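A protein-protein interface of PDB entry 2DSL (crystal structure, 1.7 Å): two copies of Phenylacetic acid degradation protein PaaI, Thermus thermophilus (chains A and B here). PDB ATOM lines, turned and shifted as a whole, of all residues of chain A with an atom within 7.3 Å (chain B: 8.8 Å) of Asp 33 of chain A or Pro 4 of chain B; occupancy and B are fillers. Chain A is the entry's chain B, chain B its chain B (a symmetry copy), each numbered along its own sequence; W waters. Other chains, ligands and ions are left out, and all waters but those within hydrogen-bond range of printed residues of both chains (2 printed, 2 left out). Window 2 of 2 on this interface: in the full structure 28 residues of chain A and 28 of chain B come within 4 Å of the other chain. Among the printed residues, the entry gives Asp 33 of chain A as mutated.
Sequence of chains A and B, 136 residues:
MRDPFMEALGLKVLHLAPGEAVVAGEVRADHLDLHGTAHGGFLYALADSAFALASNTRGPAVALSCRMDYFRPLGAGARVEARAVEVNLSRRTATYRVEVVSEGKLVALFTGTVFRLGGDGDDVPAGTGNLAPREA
No position is printed for both chains.
Of the 21 pairs that touch across the chains among the printed residues, none has its exchanged pair printed and touching as well.
OD1 of Asp 33 of chain A sits at hydrogen-bond distance from N of Gly 36 of chain A (3.2 Å).
The side-chain carboxylate of Asp 33 of chain A lies within hydrogen-bond range of the backbone NH of His 35 of chain A.
OD1 of Asp 3 of chain B sits at hydrogen-bond distance from N of Phe 5 of chain B, at 3.3 Å.
The side-chain amide oxygen of Asn 56 of chain B sits at hydrogen-bond distance from the backbone NH of Ala 61 of chain B, 3.1 Å away.
A ring nitrogen (ND1) of His 39 of chain A sits at hydrogen-bond distance from the backbone NH (N) of Gly 41 of chain A (2.8 Å).
N of Thr 37 of chain A sits at hydrogen-bond distance from OD1 of Asp 33 of chain A (3.4 Å).
Water W2 bridges OD2 of Asp 48 of chain B (2.7 Å) and N of Gly 40 of chain A (2.9 Å).
Water W1 lies within hydrogen-bond range of NE2 of His 35 of chain A (2.7 Å) and O of Ala 61 of chain B (3.4 Å).
N of Phe 5 of chain B lies within hydrogen-bond range of O of Leu 32 of chain A, at 2.9 Å.
The backbone NH of Gly 41 of chain A lies within hydrogen-bond range of the side-chain carboxylate of Asp 48 of chain B (3.5 Å).
OD2 of Asp 3 of chain B sits at hydrogen-bond distance from N of Leu 34 of chain A, at 3.0 Å.
A ring nitrogen (ND1) of His 39 of chain A lies close to the side-chain carboxylate (OD2) of Asp 48 of chain B (3.4 Å).
NE2 of His 39 of chain A sits at hydrogen-bond distance from OG of Ser 49 of chain B, 3.2 Å away.
A ring nitrogen (NE2) of His 35 of chain A lies within hydrogen-bond range of the backbone carbonyl oxygen of Ala 61 of chain B (3.1 Å).
Of the 15 printed residues of chain A, 10 touch a printed residue of chain B.
Printed residues of chain A that touch a printed residue of chain B: Ala 29, Asp 30, His 31, Leu 32, Asp 33, Leu 34, His 35, His 39, Gly 40 and Gly 41.
Hydrophobic or aromatic side chains of chain A within 4 Å of the printed part of chain B: Leu 34, His 35 and His 39.
Of the 16 printed residues of chain B, 8 touch a printed residue of chain A.
Of the printed residues of chain B, Ala 29 of chain A touches Pro 4.
Of the printed residues of chain B, Leu 32 of chain A touches Asp 3 (3.6 Å), Pro 4 (3.3 Å) and Phe 5 (2.9 Å).
Of chain B, only Asp 3 (3.3 Å) and Pro 4 (3.8 Å) come within 4 Å of Asp 33 of chain A.
Of the printed residues of chain B, Gly 41 of chain A touches Phe 5 (3.6 Å) and Asp 48 (3.5 Å).
Printed residues of chain A within 4 Å of Asp 3 of chain B: Leu 32, Asp 33, Leu 34 and His 39.
Pro 4 of chain B touches just these residues of chain A: Ala 29, Asp 30, Leu 32 and Asp 33.
Of the printed residues of chain A, Phe 5 of chain B touches Asp 30, His 31, Leu 32, His 39 and Gly 41.
Leu 11 of chain B touches none of the printed residues of chain A.
The nearest residue of chain A that does not touch Pro 4 of chain B is His 31 of chain A (4.8 Å).
The nearest printed residue of chain A that does not touch Ala 61 of chain B is Leu 34 of chain A (5.8 Å).
CB of Pro 4 of chain B touches O of Ala 29 of chain A, 3.4 Å away.
O of Asp 30 of chain A touches C of Pro 4 of chain B (3.9 Å).
Asp 30 of chain A touches Phe 5 of chain B (O to CD1, 3.2 Å).
Phe 5 of chain B touches His 31 of chain A.
Leu 32 of chain A touches Pro 4 of chain B (O to CD, 3.3 Å).
Asp 33 of chain A touches Pro 4 of chain B (O to CD, 3.8 Å).
Asn 56 of chain B touches His 35 of chain A.
CD2 of His 39 of chain A touches OD1 of Asp 3 of chain B (3.3 Å).
CA of Gly 40 of chain A touches OD2 of Asp 48 of chain B (3.6 Å).
Phe 5 of chain B touches Gly 41 of chain A.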
ATOM      1  N   ARG A  28      -5.973  -8.518 -19.857  1.00  0.00           N
ATOM      2  CA  ARG A  28      -5.290  -7.230 -19.851  1.00  0.00           C
ATOM      3  C   ARG A  28      -4.292  -7.134 -21.000  1.00  0.00           C
ATOM      4  O   ARG A  28      -4.059  -8.083 -21.743  1.00  0.00           O
ATOM      5  CB  ARG A  28      -4.533  -7.077 -18.521  1.00  0.00           C
ATOM      6  CG  ARG A  28      -5.451  -7.119 -17.290  1.00  0.00           C
ATOM      7  CD  ARG A  28      -4.666  -6.912 -15.970  1.00  0.00           C
ATOM      8  NE  ARG A  28      -3.436  -7.718 -16.011  1.00  0.00           N
ATOM      9  CZ  ARG A  28      -2.725  -7.961 -14.882  1.00  0.00           C
ATOM     10  NH1 ARG A  28      -3.106  -7.486 -13.698  1.00  0.00           N
ATOM     11  NH2 ARG A  28      -1.619  -8.696 -14.976  1.00  0.00           N
ATOM     12  N   ALA A  29      -3.722  -5.921 -21.155  1.00  0.00           N
ATOM     13  CA  ALA A  29      -2.763  -5.696 -22.231  1.00  0.00           C
ATOM     14  C   ALA A  29      -1.561  -6.635 -22.132  1.00  0.00           C
ATOM     15  O   ALA A  29      -0.944  -6.984 -23.124  1.00  0.00           O
ATOM     16  CB  ALA A  29      -2.306  -4.238 -22.188  1.00  0.00           C
ATOM     17  N   ASP A  30      -1.217  -7.016 -20.880  1.00  0.00           N
ATOM     18  CA  ASP A  30      -0.063  -7.901 -20.694  1.00  0.00           C
ATOM     19  C   ASP A  30      -0.415  -9.385 -20.818  1.00  0.00           C
ATOM     20  O   ASP A  30       0.373 -10.262 -20.482  1.00  0.00           O
ATOM     21  CB  ASP A  30       0.644  -7.583 -19.365  1.00  0.00           C
ATOM     22  CG  ASP A  30      -0.271  -7.736 -18.141  1.00  0.00           C
ATOM     23  OD1 ASP A  30      -1.437  -7.340 -18.224  1.00  0.00           O
ATOM     24  OD2 ASP A  30       0.214  -8.194 -17.106  1.00  0.00           O
ATOM     25  N   HIS A  31      -1.654  -9.647 -21.299  1.00  0.00           N
ATOM     26  CA  HIS A  31      -2.110 -11.036 -21.442  1.00  0.00           C
ATOM     27  C   HIS A  31      -2.339 -11.420 -22.909  1.00  0.00           C
ATOM     28  O   HIS A  31      -2.798 -12.516 -23.224  1.00  0.00           O
ATOM     29  CB  HIS A  31      -3.442 -11.209 -20.699  1.00  0.00           C
ATOM     30  CG  HIS A  31      -3.340 -10.943 -19.216  1.00  0.00           C
ATOM     31  ND1 HIS A  31      -4.414 -10.567 -18.471  1.00  0.00           N
ATOM     32  CD2 HIS A  31      -2.234 -11.069 -18.361  1.00  0.00           C
ATOM     33  CE1 HIS A  31      -3.966 -10.459 -17.208  1.00  0.00           C
ATOM     34  NE2 HIS A  31      -2.666 -10.753 -17.111  1.00  0.00           N
ATOM     35  N   LEU A  32      -2.058 -10.462 -23.825  1.00  0.00           N
ATOM     36  CA  LEU A  32      -2.258 -10.729 -25.245  1.00  0.00           C
ATOM     37  C   LEU A  32      -1.055 -11.451 -25.853  1.00  0.00           C
ATOM     38  O   LEU A  32       0.050 -11.438 -25.320  1.00  0.00           O
ATOM     39  CB  LEU A  32      -2.448  -9.398 -25.975  1.00  0.00           C
ATOM     40  CG  LEU A  32      -3.578  -8.555 -25.418  1.00  0.00           C
ATOM     41  CD1 LEU A  32      -3.697  -7.218 -26.174  1.00  0.00           C
ATOM     42  CD2 LEU A  32      -4.939  -9.263 -25.526  1.00  0.00           C
ATOM     43  N   ASP A  33      -1.313 -12.141 -26.991  1.00  0.00           N
ATOM     44  CA  ASP A  33      -0.248 -12.864 -27.676  1.00  0.00           C
ATOM     45  C   ASP A  33       0.074 -12.252 -29.031  1.00  0.00           C
ATOM     46  O   ASP A  33      -0.240 -11.100 -29.306  1.00  0.00           O
ATOM     47  CB  ASP A  33      -0.660 -14.346 -27.848  1.00  0.00           C
ATOM     48  CG  ASP A  33      -1.858 -14.518 -28.788  1.00  0.00           C
ATOM     49  OD1 ASP A  33      -2.258 -13.538 -29.425  1.00  0.00           O
ATOM     50  OD2 ASP A  33      -2.365 -15.635 -28.878  1.00  0.00           O
ATOM     51  N   LEU A  34       0.749 -13.067 -29.872  1.00  0.00           N
ATOM     52  CA  LEU A  34       1.159 -12.617 -31.206  1.00  0.00           C
ATOM     53  C   LEU A  34      -0.012 -12.284 -32.129  1.00  0.00           C
ATOM     54  O   LEU A  34       0.147 -11.626 -33.152  1.00  0.00           O
ATOM     55  CB  LEU A  34       2.091 -13.661 -31.829  1.00  0.00           C
ATOM     56  CG  LEU A  34       1.452 -15.005 -32.176  1.00  0.00           C
ATOM     57  CD1 LEU A  34       0.714 -14.950 -33.524  1.00  0.00           C
ATOM     58  CD2 LEU A  34       2.528 -16.103 -32.320  1.00  0.00           C
ATOM     59  N   HIS A  35      -1.205 -12.803 -31.764  1.00  0.00           N
ATOM     60  CA  HIS A  35      -2.393 -12.565 -32.593  1.00  0.00           C
ATOM     61  C   HIS A  35      -3.152 -11.308 -32.159  1.00  0.00           C
ATOM     62  O   HIS A  35      -4.032 -10.817 -32.854  1.00  0.00           O
ATOM     63  CB  HIS A  35      -3.341 -13.770 -32.480  1.00  0.00           C
ATOM     64  CG  HIS A  35      -2.718 -15.022 -33.049  1.00  0.00           C
ATOM     65  ND1 HIS A  35      -2.432 -15.190 -34.369  1.00  0.00           N
ATOM     66  CD2 HIS A  35      -2.400 -16.214 -32.377  1.00  0.00           C
ATOM     67  CE1 HIS A  35      -1.940 -16.439 -34.478  1.00  0.00           C
ATOM     68  NE2 HIS A  35      -1.909 -17.076 -33.304  1.00  0.00           N
ATOM     69  N   GLY A  36      -2.832 -10.818 -30.945  1.00  0.00           N
ATOM     70  CA  GLY A  36      -3.533  -9.636 -30.443  1.00  0.00           C
ATOM     71  C   GLY A  36      -4.728 -10.038 -29.587  1.00  0.00           C
ATOM     72  O   GLY A  36      -5.563  -9.226 -29.209  1.00  0.00           O
ATOM     73  N   THR A  37      -4.820 -11.363 -29.327  1.00  0.00           N
ATOM     74  CA  THR A  37      -5.896 -11.887 -28.498  1.00  0.00           C
ATOM     75  C   THR A  37      -5.332 -12.557 -27.253  1.00  0.00           C
ATOM     76  O   THR A  37      -4.121 -12.646 -27.064  1.00  0.00           O
ATOM     77  CB  THR A  37      -6.716 -12.907 -29.318  1.00  0.00           C
ATOM     78  OG1 THR A  37      -5.843 -13.839 -29.965  1.00  0.00           O
ATOM     79  CG2 THR A  37      -7.554 -12.195 -30.386  1.00  0.00           C
ATOM     80  N   ALA A  38      -6.242 -13.001 -26.362  1.00  0.00           N
ATOM     81  CA  ALA A  38      -5.802 -13.630 -25.117  1.00  0.00           C
ATOM     82  C   ALA A  38      -4.893 -14.831 -25.364  1.00  0.00           C
ATOM     83  O   ALA A  38      -5.226 -15.766 -26.087  1.00  0.00           O
ATOM     84  CB  ALA A  38      -7.037 -14.077 -24.331  1.00  0.00           C
ATOM     85  N   HIS A  39      -3.689 -14.764 -24.752  1.00  0.00           N
ATOM     86  CA  HIS A  39      -2.703 -15.832 -24.896  1.00  0.00           C
ATOM     87  C   HIS A  39      -3.242 -17.135 -24.302  1.00  0.00           C
ATOM     88  O   HIS A  39      -3.929 -17.149 -23.290  1.00  0.00           O
ATOM     89  CB  HIS A  39      -1.437 -15.387 -24.131  1.00  0.00           C
ATOM     90  CG  HIS A  39      -0.238 -16.250 -24.469  1.00  0.00           C
ATOM     91  ND1 HIS A  39      -0.092 -17.536 -24.042  1.00  0.00           N
ATOM     92  CD2 HIS A  39       0.926 -15.894 -25.175  1.00  0.00           C
ATOM     93  CE1 HIS A  39       1.109 -17.939 -24.498  1.00  0.00           C
ATOM     94  NE2 HIS A  39       1.742 -16.979 -25.179  1.00  0.00           N
ATOM     95  N   GLY A  40      -2.947 -18.242 -25.001  1.00  0.00           N
ATOM     96  CA  GLY A  40      -3.422 -19.542 -24.534  1.00  0.00           C
ATOM     97  C   GLY A  40      -2.975 -19.827 -23.100  1.00  0.00           C
ATOM     98  O   GLY A  40      -3.627 -20.537 -22.350  1.00  0.00           O
ATOM     99  N   GLY A  41      -1.797 -19.273 -22.748  1.00  0.00           N
ATOM    100  CA  GLY A  41      -1.251 -19.502 -21.414  1.00  0.00           C
ATOM    101  C   GLY A  41      -2.037 -18.760 -20.334  1.00  0.00           C
ATOM    102  O   GLY A  41      -2.087 -19.169 -19.180  1.00  0.00           O
ATOM    103  N   LEU A  74     -10.265 -14.538 -27.623  1.00  0.00           N
ATOM    104  CA  LEU A  74     -10.847 -13.405 -26.906  1.00  0.00           C
ATOM    105  C   LEU A  74     -10.016 -12.141 -27.090  1.00  0.00           C
ATOM    106  O   LEU A  74      -8.790 -12.157 -27.098  1.00  0.00           O
ATOM    107  CB  LEU A  74     -10.870 -13.714 -25.412  1.00  0.00           C
ATOM    108  CG  LEU A  74     -11.637 -14.964 -25.045  1.00  0.00           C
ATOM    109  CD1 LEU A  74     -11.669 -15.139 -23.513  1.00  0.00           C
ATOM    110  CD2 LEU A  74     -13.094 -14.921 -25.525  1.00  0.00           C
ATOM    111  N   ASP B   3       5.301 -10.511 -28.373  1.00  0.00           N
ATOM    112  CA  ASP B   3       4.227 -11.213 -27.615  1.00  0.00           C
ATOM    113  C   ASP B   3       4.165 -10.654 -26.198  1.00  0.00           C
ATOM    114  O   ASP B   3       5.038 -10.926 -25.377  1.00  0.00           O
ATOM    115  CB  ASP B   3       4.516 -12.711 -27.569  1.00  0.00           C
ATOM    116  CG  ASP B   3       3.330 -13.514 -27.097  1.00  0.00           C
ATOM    117  OD1 ASP B   3       2.964 -13.421 -25.906  1.00  0.00           O
ATOM    118  OD2 ASP B   3       2.755 -14.237 -27.933  1.00  0.00           O
ATOM    119  N   PRO B   4       3.127  -9.860 -25.899  1.00  0.00           N
ATOM    120  CA  PRO B   4       2.960  -9.260 -24.575  1.00  0.00           C
ATOM    121  C   PRO B   4       3.031 -10.212 -23.386  1.00  0.00           C
ATOM    122  O   PRO B   4       3.777  -9.961 -22.442  1.00  0.00           O
ATOM    123  CB  PRO B   4       1.607  -8.567 -24.688  1.00  0.00           C
ATOM    124  CG  PRO B   4       1.608  -8.111 -26.112  1.00  0.00           C
ATOM    125  CD  PRO B   4       2.105  -9.348 -26.830  1.00  0.00           C
ATOM    126  N   PHE B   5       2.260 -11.296 -23.420  1.00  0.00           N
ATOM    127  CA  PHE B   5       2.261 -12.233 -22.303  1.00  0.00           C
ATOM    128  C   PHE B   5       3.640 -12.862 -22.128  1.00  0.00           C
ATOM    129  O   PHE B   5       4.111 -13.035 -21.007  1.00  0.00           O
ATOM    130  CB  PHE B   5       1.194 -13.318 -22.510  1.00  0.00           C
ATOM    131  CG  PHE B   5       0.871 -14.098 -21.263  1.00  0.00           C
ATOM    132  CD1 PHE B   5       0.572 -13.440 -20.073  1.00  0.00           C
ATOM    133  CD2 PHE B   5       0.844 -15.491 -21.283  1.00  0.00           C
ATOM    134  CE1 PHE B   5       0.251 -14.159 -18.919  1.00  0.00           C
ATOM    135  CE2 PHE B   5       0.523 -16.217 -20.139  1.00  0.00           C
ATOM    136  CZ  PHE B   5       0.226 -15.552 -18.956  1.00  0.00           C
ATOM    137  N   MET B   6       4.291 -13.198 -23.237  1.00  0.00           N
ATOM    138  CA  MET B   6       5.629 -13.776 -23.166  1.00  0.00           C
ATOM    139  C   MET B   6       6.574 -12.833 -22.440  1.00  0.00           C
ATOM    140  O   MET B   6       7.299 -13.242 -21.534  1.00  0.00           O
ATOM    141  CB  MET B   6       6.184 -14.039 -24.562  1.00  0.00           C
ATOM    142  CG  MET B   6       5.635 -15.268 -25.238  1.00  0.00           C
ATOM    143  SD  MET B   6       6.576 -15.603 -26.735  1.00  0.00           S
ATOM    144  CE  MET B   6       8.115 -16.069 -26.056  1.00  0.00           C
ATOM    145  N   GLU B   7       6.566 -11.567 -22.847  1.00  0.00           N
ATOM    146  CA  GLU B   7       7.439 -10.571 -22.239  1.00  0.00           C
ATOM    147  C   GLU B   7       7.105 -10.364 -20.773  1.00  0.00           C
ATOM    148  O   GLU B   7       7.998 -10.245 -19.940  1.00  0.00           O
ATOM    149  CB  GLU B   7       7.328  -9.228 -22.967  1.00  0.00           C
ATOM    150  CG  GLU B   7       7.642  -9.283 -24.449  1.00  0.00           C
ATOM    151  CD  GLU B   7       8.020  -7.925 -25.009  1.00  0.00           C
ATOM    152  OE1 GLU B   7       7.333  -6.929 -24.699  1.00  0.00           O
ATOM    153  OE2 GLU B   7       9.008  -7.858 -25.771  1.00  0.00           O
ATOM    154  N   ALA B   8       5.814 -10.317 -20.461  1.00  0.00           N
ATOM    155  CA  ALA B   8       5.377 -10.112 -19.087  1.00  0.00           C
ATOM    156  C   ALA B   8       5.846 -11.233 -18.168  1.00  0.00           C
ATOM    157  O   ALA B   8       5.991 -11.035 -16.959  1.00  0.00           O
ATOM    158  CB  ALA B   8       3.858  -9.994 -19.035  1.00  0.00           C
ATOM    159  N   LEU B   9       6.079 -12.413 -18.739  1.00  0.00           N
ATOM    160  CA  LEU B   9       6.534 -13.556 -17.952  1.00  0.00           C
ATOM    161  C   LEU B   9       8.054 -13.702 -17.963  1.00  0.00           C
ATOM    162  O   LEU B   9       8.600 -14.616 -17.343  1.00  0.00           O
ATOM    163  CB  LEU B   9       5.886 -14.852 -18.459  1.00  0.00           C
ATOM    164  CG  LEU B   9       4.541 -15.231 -17.822  1.00  0.00           C
ATOM    165  CD1 LEU B   9       3.611 -14.031 -17.769  1.00  0.00           C
ATOM    166  CD2 LEU B   9       3.915 -16.368 -18.609  1.00  0.00           C
ATOM    167  N   GLY B  10       8.727 -12.796 -18.664  1.00  0.00           N
ATOM    168  CA  GLY B  10      10.179 -12.828 -18.728  1.00  0.00           C
ATOM    169  C   GLY B  10      10.751 -13.890 -19.645  1.00  0.00           C
ATOM    170  O   GLY B  10      11.932 -14.234 -19.544  1.00  0.00           O
ATOM    171  N   LEU B  11       9.924 -14.406 -20.549  1.00  0.00           N
ATOM    172  CA  LEU B  11      10.359 -15.451 -21.469  1.00  0.00           C
ATOM    173  C   LEU B  11      11.146 -14.903 -22.653  1.00  0.00           C
ATOM    174  O   LEU B  11      10.886 -13.799 -23.146  1.00  0.00           O
ATOM    175  CB  LEU B  11       9.148 -16.239 -21.970  1.00  0.00           C
ATOM    176  CG  LEU B  11       8.202 -16.720 -20.864  1.00  0.00           C
ATOM    177  CD1 LEU B  11       7.075 -17.537 -21.482  1.00  0.00           C
ATOM    178  CD2 LEU B  11       8.973 -17.545 -19.842  1.00  0.00           C
ATOM    179  N   ASP B  48       3.444 -23.395 -24.171  1.00  0.00           N
ATOM    180  CA  ASP B  48       2.502 -22.880 -25.164  1.00  0.00           C
ATOM    181  C   ASP B  48       3.139 -21.807 -26.049  1.00  0.00           C
ATOM    182  O   ASP B  48       2.826 -21.681 -27.221  1.00  0.00           O
ATOM    183  CB  ASP B  48       1.285 -22.320 -24.418  1.00  0.00           C
ATOM    184  CG  ASP B  48       0.216 -21.851 -25.405  1.00  0.00           C
ATOM    185  OD1 ASP B  48      -0.339 -22.702 -26.110  1.00  0.00           O
ATOM    186  OD2 ASP B  48      -0.071 -20.655 -25.433  1.00  0.00           O
ATOM    187  N   SER B  49       4.029 -20.993 -25.437  1.00  0.00           N
ATOM    188  CA  SER B  49       4.675 -19.945 -26.229  1.00  0.00           C
ATOM    189  C   SER B  49       5.583 -20.542 -27.304  1.00  0.00           C
ATOM    190  O   SER B  49       5.654 -20.058 -28.425  1.00  0.00           O
ATOM    191  CB  SER B  49       5.476 -19.022 -25.305  1.00  0.00           C
ATOM    192  OG  SER B  49       4.578 -18.280 -24.469  1.00  0.00           O
ATOM    193  N   ALA B  52       3.315 -21.887 -29.913  1.00  0.00           N
ATOM    194  CA  ALA B  52       2.779 -20.846 -30.788  1.00  0.00           C
ATOM    195  C   ALA B  52       3.802 -20.400 -31.832  1.00  0.00           C
ATOM    196  O   ALA B  52       3.489 -20.206 -32.996  1.00  0.00           O
ATOM    197  CB  ALA B  52       2.348 -19.656 -29.927  1.00  0.00           C
ATOM    198  N   ASN B  56       3.446 -21.206 -35.847  1.00  0.00           N
ATOM    199  CA  ASN B  56       3.203 -20.063 -36.730  1.00  0.00           C
ATOM    200  C   ASN B  56       4.316 -19.842 -37.777  1.00  0.00           C
ATOM    201  O   ASN B  56       4.207 -18.967 -38.634  1.00  0.00           O
ATOM    202  CB  ASN B  56       2.981 -18.808 -35.877  1.00  0.00           C
ATOM    203  CG  ASN B  56       1.523 -18.710 -35.466  1.00  0.00           C
ATOM    204  OD1 ASN B  56       0.693 -18.108 -36.138  1.00  0.00           O
ATOM    205  ND2 ASN B  56       1.209 -19.315 -34.302  1.00  0.00           N
ATOM    206  N   ALA B  61      -1.670 -19.700 -37.351  1.00  0.00           N
ATOM    207  CA  ALA B  61      -2.307 -20.874 -36.766  1.00  0.00           C
ATOM    208  C   ALA B  61      -2.777 -20.588 -35.349  1.00  0.00           C
ATOM    209  O   ALA B  61      -2.136 -19.872 -34.586  1.00  0.00           O
ATOM    210  CB  ALA B  61      -1.284 -22.019 -36.732  1.00  0.00           C
ATOM    211  N   VAL B  62      -3.972 -21.132 -35.023  1.00  0.00           N
ATOM    212  CA  VAL B  62      -4.530 -20.973 -33.682  1.00  0.00           C
ATOM    213  C   VAL B  62      -4.695 -22.323 -33.008  1.00  0.00           C
ATOM    214  O   VAL B  62      -4.997 -23.329 -33.639  1.00  0.00           O
ATOM    215  CB  VAL B  62      -5.910 -20.300 -33.776  1.00  0.00           C
ATOM    216  CG1 VAL B  62      -5.785 -18.872 -34.300  1.00  0.00           C
ATOM    217  CG2 VAL B  62      -6.847 -21.100 -34.667  1.00  0.00           C
ATOM    218  N   ALA B  63      -4.457 -22.332 -31.682  1.00  0.00           N
ATOM    219  CA  ALA B  63      -4.535 -23.582 -30.930  1.00  0.00           C
ATOM    220  C   ALA B  63      -5.963 -24.112 -30.798  1.00  0.00           C
ATOM    221  O   ALA B  63      -6.927 -23.377 -30.619  1.00  0.00           O
ATOM    222  CB  ALA B  63      -3.963 -23.337 -29.534  1.00  0.00           C
HETATM  223  O   HOH W   1      -1.232 -18.974 -31.441  1.00  0.00           O
HETATM  224  O   HOH W   2      -1.240 -18.998 -27.213  1.00  0.00           O
